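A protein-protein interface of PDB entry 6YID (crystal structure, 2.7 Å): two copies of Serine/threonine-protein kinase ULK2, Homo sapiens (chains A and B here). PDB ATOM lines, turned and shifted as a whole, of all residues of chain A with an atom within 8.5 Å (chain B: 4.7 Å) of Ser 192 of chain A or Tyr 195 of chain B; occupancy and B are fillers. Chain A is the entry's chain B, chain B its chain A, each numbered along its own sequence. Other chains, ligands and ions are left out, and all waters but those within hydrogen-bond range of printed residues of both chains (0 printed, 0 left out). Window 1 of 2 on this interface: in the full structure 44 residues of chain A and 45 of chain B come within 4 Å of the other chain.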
ATOM      1  N   ARG A 134     -10.618 -24.762  12.293  1.00  0.00           N
ATOM      2  CA  ARG A 134     -11.221 -24.800  13.645  1.00  0.00           C
ATOM      3  C   ARG A 134     -11.579 -26.221  14.105  1.00  0.00           C
ATOM      4  O   ARG A 134     -11.963 -26.402  15.249  1.00  0.00           O
ATOM      5  CB  ARG A 134     -12.463 -23.912  13.715  1.00  0.00           C
ATOM      6  CG  ARG A 134     -12.183 -22.456  13.365  1.00  0.00           C
ATOM      7  CD  ARG A 134     -13.082 -21.529  14.125  1.00  0.00           C
ATOM      8  NE  ARG A 134     -14.474 -21.830  13.888  1.00  0.00           N
ATOM      9  CZ  ARG A 134     -15.464 -21.397  14.635  1.00  0.00           C
ATOM     10  NH1 ARG A 134     -15.209 -20.602  15.667  1.00  0.00           N
ATOM     11  NH2 ARG A 134     -16.698 -21.771  14.346  1.00  0.00           N
ATOM     12  N   ARG A 167     -14.227 -20.915   9.020  1.00  0.00           N
ATOM     13  CA  ARG A 167     -14.766 -19.567   8.863  1.00  0.00           C
ATOM     14  C   ARG A 167     -13.675 -18.676   8.294  1.00  0.00           C
ATOM     15  O   ARG A 167     -12.483 -19.010   8.356  1.00  0.00           O
ATOM     16  CB  ARG A 167     -15.369 -19.040  10.173  1.00  0.00           C
ATOM     17  CG  ARG A 167     -14.403 -18.284  11.070  1.00  0.00           C
ATOM     18  CD  ARG A 167     -15.033 -17.813  12.376  1.00  0.00           C
ATOM     19  NE  ARG A 167     -14.152 -16.954  13.151  1.00  0.00           N
ATOM     20  CZ  ARG A 167     -13.872 -15.681  12.865  1.00  0.00           C
ATOM     21  NH1 ARG A 167     -14.556 -15.019  11.955  1.00  0.00           N
ATOM     22  NH2 ARG A 167     -12.889 -15.066  13.489  1.00  0.00           N
ATOM     23  N   LEU A 169     -11.729 -15.032   8.255  1.00  0.00           N
ATOM     24  CA  LEU A 169     -11.336 -13.871   9.071  1.00  0.00           C
ATOM     25  C   LEU A 169     -11.802 -12.591   8.392  1.00  0.00           C
ATOM     26  O   LEU A 169     -11.408 -12.328   7.265  1.00  0.00           O
ATOM     27  CB  LEU A 169      -9.814 -13.840   9.207  1.00  0.00           C
ATOM     28  CG  LEU A 169      -9.229 -14.800  10.239  1.00  0.00           C
ATOM     29  CD1 LEU A 169      -7.719 -14.634  10.316  1.00  0.00           C
ATOM     30  CD2 LEU A 169      -9.868 -14.575  11.603  1.00  0.00           C
ATOM     31  N   MET A 185     -23.053  -2.333  17.263  1.00  0.00           N
ATOM     32  CA  MET A 185     -22.628  -3.688  17.385  1.00  0.00           C
ATOM     33  C   MET A 185     -22.175  -3.967  18.829  1.00  0.00           C
ATOM     34  O   MET A 185     -21.543  -3.149  19.464  1.00  0.00           O
ATOM     35  CB  MET A 185     -21.505  -3.967  16.390  1.00  0.00           C
ATOM     36  CG  MET A 185     -21.331  -5.434  16.073  1.00  0.00           C
ATOM     37  SD  MET A 185     -20.102  -5.715  14.767  1.00  0.00           S
ATOM     38  CE  MET A 185     -20.966  -5.023  13.355  1.00  0.00           C
ATOM     39  N   ALA A 186     -22.515  -5.155  19.326  1.00  0.00           N
ATOM     40  CA  ALA A 186     -22.227  -5.579  20.696  1.00  0.00           C
ATOM     41  C   ALA A 186     -20.726  -5.616  20.903  1.00  0.00           C
ATOM     42  O   ALA A 186     -19.989  -6.101  20.058  1.00  0.00           O
ATOM     43  CB  ALA A 186     -22.841  -6.925  20.991  1.00  0.00           C
ATOM     44  N   PRO A 187     -20.229  -5.097  22.043  1.00  0.00           N
ATOM     45  CA  PRO A 187     -18.794  -5.046  22.306  1.00  0.00           C
ATOM     46  C   PRO A 187     -18.098  -6.406  22.215  1.00  0.00           C
ATOM     47  O   PRO A 187     -16.967  -6.481  21.756  1.00  0.00           O
ATOM     48  CB  PRO A 187     -18.729  -4.495  23.737  1.00  0.00           C
ATOM     49  CG  PRO A 187     -20.006  -3.691  23.878  1.00  0.00           C
ATOM     50  CD  PRO A 187     -21.023  -4.509  23.135  1.00  0.00           C
ATOM     51  N   GLU A 188     -18.767  -7.467  22.666  1.00  0.00           N
ATOM     52  CA  GLU A 188     -18.168  -8.804  22.627  1.00  0.00           C
ATOM     53  C   GLU A 188     -17.862  -9.176  21.166  1.00  0.00           C
ATOM     54  O   GLU A 188     -16.862  -9.775  20.882  1.00  0.00           O
ATOM     55  CB  GLU A 188     -19.043  -9.838  23.351  1.00  0.00           C
ATOM     56  CG  GLU A 188     -20.429 -10.021  22.787  1.00  0.00           C
ATOM     57  CD  GLU A 188     -21.563  -9.355  23.569  1.00  0.00           C
ATOM     58  OE1 GLU A 188     -21.352  -8.231  24.048  1.00  0.00           O
ATOM     59  OE2 GLU A 188     -22.675  -9.961  23.664  1.00  0.00           O
ATOM     60  N   VAL A 189     -18.705  -8.717  20.242  1.00  0.00           N
ATOM     61  CA  VAL A 189     -18.566  -9.028  18.823  1.00  0.00           C
ATOM     62  C   VAL A 189     -17.427  -8.201  18.229  1.00  0.00           C
ATOM     63  O   VAL A 189     -16.589  -8.742  17.525  1.00  0.00           O
ATOM     64  CB  VAL A 189     -19.880  -8.790  18.062  1.00  0.00           C
ATOM     65  CG1 VAL A 189     -19.684  -8.999  16.577  1.00  0.00           C
ATOM     66  CG2 VAL A 189     -21.018  -9.663  18.587  1.00  0.00           C
ATOM     67  N   ILE A 190     -17.411  -6.892  18.507  1.00  0.00           N
ATOM     68  CA  ILE A 190     -16.312  -6.013  18.076  1.00  0.00           C
ATOM     69  C   ILE A 190     -14.976  -6.638  18.508  1.00  0.00           C
ATOM     70  O   ILE A 190     -14.058  -6.788  17.704  1.00  0.00           O
ATOM     71  CB  ILE A 190     -16.423  -4.608  18.682  1.00  0.00           C
ATOM     72  CG1 ILE A 190     -17.773  -3.926  18.448  1.00  0.00           C
ATOM     73  CG2 ILE A 190     -15.252  -3.754  18.204  1.00  0.00           C
ATOM     74  CD1 ILE A 190     -17.956  -3.452  17.069  1.00  0.00           C
ATOM     75  N   MET A 191     -14.890  -6.960  19.807  1.00  0.00           N
ATOM     76  CA  MET A 191     -13.649  -7.302  20.472  1.00  0.00           C
ATOM     77  C   MET A 191     -13.210  -8.726  20.111  1.00  0.00           C
ATOM     78  O   MET A 191     -12.042  -9.057  20.276  1.00  0.00           O
ATOM     79  CB  MET A 191     -13.794  -7.228  21.995  1.00  0.00           C
ATOM     80  CG  MET A 191     -13.886  -5.831  22.559  1.00  0.00           C
ATOM     81  SD  MET A 191     -13.774  -5.883  24.363  1.00  0.00           S
ATOM     82  CE  MET A 191     -15.347  -6.598  24.842  1.00  0.00           C
ATOM     83  N   SER A 192     -14.139  -9.569  19.647  1.00  0.00           N
ATOM     84  CA  SER A 192     -13.839 -10.984  19.433  1.00  0.00           C
ATOM     85  C   SER A 192     -13.301 -11.231  18.020  1.00  0.00           C
ATOM     86  O   SER A 192     -12.955 -12.339  17.720  1.00  0.00           O
ATOM     87  CB  SER A 192     -15.035 -11.843  19.690  1.00  0.00           C
ATOM     88  OG  SER A 192     -15.969 -11.725  18.621  1.00  0.00           O
ATOM     89  N   GLN A 193     -13.201 -10.195  17.191  1.00  0.00           N
ATOM     90  CA  GLN A 193     -12.595 -10.336  15.871  1.00  0.00           C
ATOM     91  C   GLN A 193     -11.171 -10.896  16.019  1.00  0.00           C
ATOM     92  O   GLN A 193     -10.411 -10.443  16.857  1.00  0.00           O
ATOM     93  CB  GLN A 193     -12.596  -8.986  15.152  1.00  0.00           C
ATOM     94  CG  GLN A 193     -12.918  -9.088  13.676  1.00  0.00           C
ATOM     95  CD  GLN A 193     -13.376  -7.762  13.110  1.00  0.00           C
ATOM     96  OE1 GLN A 193     -14.555  -7.575  12.796  1.00  0.00           O
ATOM     97  NE2 GLN A 193     -12.447  -6.823  13.001  1.00  0.00           N
ATOM     98  N   HIS A 194     -10.848 -11.918  15.225  1.00  0.00           N
ATOM     99  CA  HIS A 194      -9.486 -12.517  15.153  1.00  0.00           C
ATOM    100  C   HIS A 194      -9.133 -13.367  16.393  1.00  0.00           C
ATOM    101  O   HIS A 194      -8.018 -13.815  16.498  1.00  0.00           O
ATOM    102  CB  HIS A 194      -8.428 -11.432  14.897  1.00  0.00           C
ATOM    103  CG  HIS A 194      -8.428 -10.900  13.499  1.00  0.00           C
ATOM    104  ND1 HIS A 194      -7.288 -10.367  12.905  1.00  0.00           N
ATOM    105  CD2 HIS A 194      -9.397 -10.846  12.554  1.00  0.00           C
ATOM    106  CE1 HIS A 194      -7.575  -9.973  11.680  1.00  0.00           C
ATOM    107  NE2 HIS A 194      -8.864 -10.250  11.442  1.00  0.00           N
ATOM    108  N   TYR A 195     -10.088 -13.610  17.305  1.00  0.00           N
ATOM    109  CA  TYR A 195      -9.791 -14.297  18.600  1.00  0.00           C
ATOM    110  C   TYR A 195      -9.290 -15.726  18.327  1.00  0.00           C
ATOM    111  O   TYR A 195      -8.441 -16.231  19.044  1.00  0.00           O
ATOM    112  CB  TYR A 195     -11.011 -14.294  19.539  1.00  0.00           C
ATOM    113  CG  TYR A 195     -11.996 -15.404  19.302  1.00  0.00           C
ATOM    114  CD1 TYR A 195     -12.944 -15.305  18.299  1.00  0.00           C
ATOM    115  CD2 TYR A 195     -11.955 -16.578  20.030  1.00  0.00           C
ATOM    116  CE1 TYR A 195     -13.840 -16.328  18.028  1.00  0.00           C
ATOM    117  CE2 TYR A 195     -12.838 -17.619  19.771  1.00  0.00           C
ATOM    118  CZ  TYR A 195     -13.786 -17.491  18.765  1.00  0.00           C
ATOM    119  OH  TYR A 195     -14.643 -18.508  18.476  1.00  0.00           O
ATOM    120  N   ASP A 196      -9.820 -16.353  17.268  1.00  0.00           N
ATOM    121  CA  ASP A 196      -9.560 -17.746  16.941  1.00  0.00           C
ATOM    122  C   ASP A 196      -8.583 -17.853  15.757  1.00  0.00           C
ATOM    123  O   ASP A 196      -8.473 -18.912  15.141  1.00  0.00           O
ATOM    124  CB  ASP A 196     -10.859 -18.503  16.657  1.00  0.00           C
ATOM    125  CG  ASP A 196     -11.724 -17.934  15.525  1.00  0.00           C
ATOM    126  OD1 ASP A 196     -11.390 -16.840  15.001  1.00  0.00           O
ATOM    127  OD2 ASP A 196     -12.744 -18.580  15.190  1.00  0.00           O
ATOM    128  N   ALA A 197      -7.827 -16.781  15.493  1.00  0.00           N
ATOM    129  CA  ALA A 197      -6.953 -16.701  14.314  1.00  0.00           C
ATOM    130  C   ALA A 197      -5.858 -17.784  14.343  1.00  0.00           C
ATOM    131  O   ALA A 197      -5.358 -18.175  13.289  1.00  0.00           O
ATOM    132  CB  ALA A 197      -6.367 -15.316  14.204  1.00  0.00           C
ATOM    133  N   GLN A 260      -3.530 -17.510  22.975  1.00  0.00           N
ATOM    134  CA  GLN A 260      -3.159 -17.220  21.584  1.00  0.00           C
ATOM    135  C   GLN A 260      -2.137 -16.072  21.566  1.00  0.00           C
ATOM    136  O   GLN A 260      -1.267 -16.031  20.702  1.00  0.00           O
ATOM    137  CB  GLN A 260      -4.415 -16.940  20.735  1.00  0.00           C
ATOM    138  CG  GLN A 260      -5.286 -15.776  21.205  1.00  0.00           C
ATOM    139  CD  GLN A 260      -6.485 -16.188  22.039  1.00  0.00           C
ATOM    140  OE1 GLN A 260      -6.392 -16.993  22.968  1.00  0.00           O
ATOM    141  NE2 GLN A 260      -7.633 -15.600  21.737  1.00  0.00           N
ATOM    142  N   ARG B 134     -26.494 -10.227  15.179  1.00  0.00           N
ATOM    143  CA  ARG B 134     -25.140  -9.684  15.410  1.00  0.00           C
ATOM    144  C   ARG B 134     -24.918  -8.334  14.712  1.00  0.00           C
ATOM    145  O   ARG B 134     -23.926  -7.677  14.980  1.00  0.00           O
ATOM    146  CB  ARG B 134     -24.050 -10.670  14.983  1.00  0.00           C
ATOM    147  CG  ARG B 134     -24.133 -12.007  15.697  1.00  0.00           C
ATOM    148  CD  ARG B 134     -22.778 -12.648  15.856  1.00  0.00           C
ATOM    149  NE  ARG B 134     -22.072 -12.781  14.596  1.00  0.00           N
ATOM    150  CZ  ARG B 134     -20.767 -12.942  14.483  1.00  0.00           C
ATOM    151  NH1 ARG B 134     -20.005 -13.030  15.563  1.00  0.00           N
ATOM    152  NH2 ARG B 134     -20.234 -13.008  13.279  1.00  0.00           N
ATOM    153  N   SER B 192     -15.079 -19.905  24.078  1.00  0.00           N
ATOM    154  CA  SER B 192     -15.800 -18.771  23.495  1.00  0.00           C
ATOM    155  C   SER B 192     -17.225 -19.164  23.077  1.00  0.00           C
ATOM    156  O   SER B 192     -17.940 -18.351  22.498  1.00  0.00           O
ATOM    157  CB  SER B 192     -15.062 -18.209  22.321  1.00  0.00           C
ATOM    158  OG  SER B 192     -15.221 -19.051  21.188  1.00  0.00           O
ATOM    159  N   GLN B 193     -17.625 -20.409  23.318  1.00  0.00           N
ATOM    160  CA  GLN B 193     -18.978 -20.840  22.988  1.00  0.00           C
ATOM    161  C   GLN B 193     -19.981 -19.940  23.728  1.00  0.00           C
ATOM    162  O   GLN B 193     -19.793 -19.666  24.897  1.00  0.00           O
ATOM    163  CB  GLN B 193     -19.153 -22.321  23.331  1.00  0.00           C
ATOM    164  CG  GLN B 193     -20.045 -23.065  22.345  1.00  0.00           C
ATOM    165  CD  GLN B 193     -19.912 -24.558  22.483  1.00  0.00           C
ATOM    166  OE1 GLN B 193     -19.324 -25.226  21.636  1.00  0.00           O
ATOM    167  NE2 GLN B 193     -20.448 -25.086  23.573  1.00  0.00           N
ATOM    168  N   HIS B 194     -21.003 -19.443  23.014  1.00  0.00           N
ATOM    169  CA  HIS B 194     -22.110 -18.641  23.592  1.00  0.00           C
ATOM    170  C   HIS B 194     -21.668 -17.217  23.992  1.00  0.00           C
ATOM    171  O   HIS B 194     -22.434 -16.501  24.635  1.00  0.00           O
ATOM    172  CB  HIS B 194     -22.731 -19.368  24.799  1.00  0.00           C
ATOM    173  CG  HIS B 194     -23.573 -20.545  24.439  1.00  0.00           C
ATOM    174  ND1 HIS B 194     -24.529 -21.056  25.302  1.00  0.00           N
ATOM    175  CD2 HIS B 194     -23.636 -21.297  23.314  1.00  0.00           C
ATOM    176  CE1 HIS B 194     -25.128 -22.087  24.737  1.00  0.00           C
ATOM    177  NE2 HIS B 194     -24.607 -22.249  23.515  1.00  0.00           N
ATOM    178  N   TYR B 195     -20.462 -16.787  23.601  1.00  0.00           N
ATOM    179  CA  TYR B 195     -19.920 -15.477  24.036  1.00  0.00           C
ATOM    180  C   TYR B 195     -20.804 -14.337  23.504  1.00  0.00           C
ATOM    181  O   TYR B 195     -20.982 -13.314  24.178  1.00  0.00           O
ATOM    182  CB  TYR B 195     -18.455 -15.282  23.612  1.00  0.00           C
ATOM    183  CG  TYR B 195     -18.262 -14.780  22.205  1.00  0.00           C
ATOM    184  CD1 TYR B 195     -18.321 -15.649  21.138  1.00  0.00           C
ATOM    185  CD2 TYR B 195     -18.067 -13.439  21.934  1.00  0.00           C
ATOM    186  CE1 TYR B 195     -18.184 -15.212  19.832  1.00  0.00           C
ATOM    187  CE2 TYR B 195     -17.917 -12.979  20.636  1.00  0.00           C
ATOM    188  CZ  TYR B 195     -17.969 -13.874  19.577  1.00  0.00           C
ATOM    189  OH  TYR B 195     -17.832 -13.498  18.272  1.00  0.00           O
ATOM    190  N   ASP B 196     -21.366 -14.529  22.301  1.00  0.00           N
ATOM    191  CA  ASP B 196     -22.131 -13.499  21.615  1.00  0.00           C
ATOM    192  C   ASP B 196     -23.633 -13.803  21.702  1.00  0.00           C
ATOM    193  O   ASP B 196     -24.417 -13.234  20.961  1.00  0.00           O
ATOM    194  CB  ASP B 196     -21.657 -13.335  20.165  1.00  0.00           C
ATOM    195  CG  ASP B 196     -21.749 -14.582  19.297  1.00  0.00           C
ATOM    196  OD1 ASP B 196     -22.062 -15.681  19.841  1.00  0.00           O
ATOM    197  OD2 ASP B 196     -21.489 -14.454  18.076  1.00  0.00           O
ATOM    198  N   ALA B 197     -24.031 -14.644  22.660  1.00  0.00           N
ATOM    199  CA  ALA B 197     -25.419 -15.117  22.788  1.00  0.00           C
ATOM    200  C   ALA B 197     -26.380 -13.952  23.068  1.00  0.00           C
ATOM    201  O   ALA B 197     -27.561 -14.045  22.720  1.00  0.00           O
ATOM    202  CB  ALA B 197     -25.517 -16.162  23.872  1.00  0.00           C
ATOM    203  N   GLN B 260     -21.697  -9.271  29.012  1.00  0.00           N
ATOM    204  CA  GLN B 260     -22.836 -10.144  28.690  1.00  0.00           C
ATOM    205  C   GLN B 260     -23.268 -10.902  29.956  1.00  0.00           C
ATOM    206  O   GLN B 260     -24.446 -11.216  30.157  1.00  0.00           O
ATOM    207  CB  GLN B 260     -22.484 -11.079  27.521  1.00  0.00           C
ATOM    208  CG  GLN B 260     -21.251 -11.966  27.728  1.00  0.00           C
ATOM    209  CD  GLN B 260     -19.983 -11.428  27.078  1.00  0.00           C
ATOM    210  OE1 GLN B 260     -19.598 -10.275  27.269  1.00  0.00           O
ATOM    211  NE2 GLN B 260     -19.297 -12.269  26.312  1.00  0.00           N
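Of the 17 printed residues of chain A, 4 touch a printed residue of chain B.
Hydrophobic or aromatic side chains of chain A that line the printed part of chain B: Met 185 and Tyr 195.
Printed residues of chain B that touch a printed residue of chain A: Arg 134, Ser 192, Tyr 195 and Gln 260.
Hydrophobic or aromatic side chains of chain B that line the printed part of chain A: Tyr 195.
Among the printed residues, no Asp or Glu carboxylate lies within 4 Å of a Lys or Arg side-chain nitrogen of the other chain.
OG of Ser 192 of chain B sits at hydrogen-bond distance from OH of Tyr 195 of chain A, 2.8 Å away.
OG of Ser 192 of chain A sits at hydrogen-bond distance from OH of Tyr 195 of chain B (2.6 Å).
Met 185 of chain A touches Arg 134 of chain B.
Tyr 195 of chain B touches Glu 188 of chain A (CE2 to O, 3.4 Å).
CB of Glu 188 of chain A touches NE2 of Gln 260 of chain B (3.8 Å).
The guanidinium group (NH1) of Arg 134 of chain B lies within salt-bridge range of the side-chain carboxylate (OD2) of Asp 196 of chain B, at 3.2 Å.
O of Tyr 195 of chain A sits at hydrogen-bond distance from NE2 of Gln 260 of chain A, at 2.9 Å.
The backbone carbonyl oxygen (O) of Tyr 195 of chain B lies within hydrogen-bond range of the side-chain amide nitrogen (NE2) of Gln 260 of chain B.
O of Val 189 of chain A is in hydrogen-bond range of OG of Ser 192 of chain A (3.2 Å).
The backbone carbonyl oxygen of Glu 188 of chain A sits close to the side-chain hydroxyl of Ser 192 of chain A (3.1 Å).
Leu 169 of chain A touches none of the printed residues of chain B.
Printed residues of chain B within 4 Å of Glu 188 of chain A: Tyr 195 and Gln 260.
Ser 192 of chain A touches just one residue of chain B: Tyr 195.
Printed residues of chain B within 4 Å of Tyr 195 of chain A: Ser 192.
Asp 196 of chain A touches none of the printed residues of chain B.
Tyr 195 of chain B touches just these residues of chain A: Glu 188 and Ser 192.
The nearest residue of chain A that does not touch Tyr 195 of chain B is Val 189 of chain A (4.4 Å).
Ser 192 of chain A touches Tyr 195 of chain B, and with the chains exchanged Tyr 195 of chain A touches Ser 192 of chain B.
8 positions are printed for both chains.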
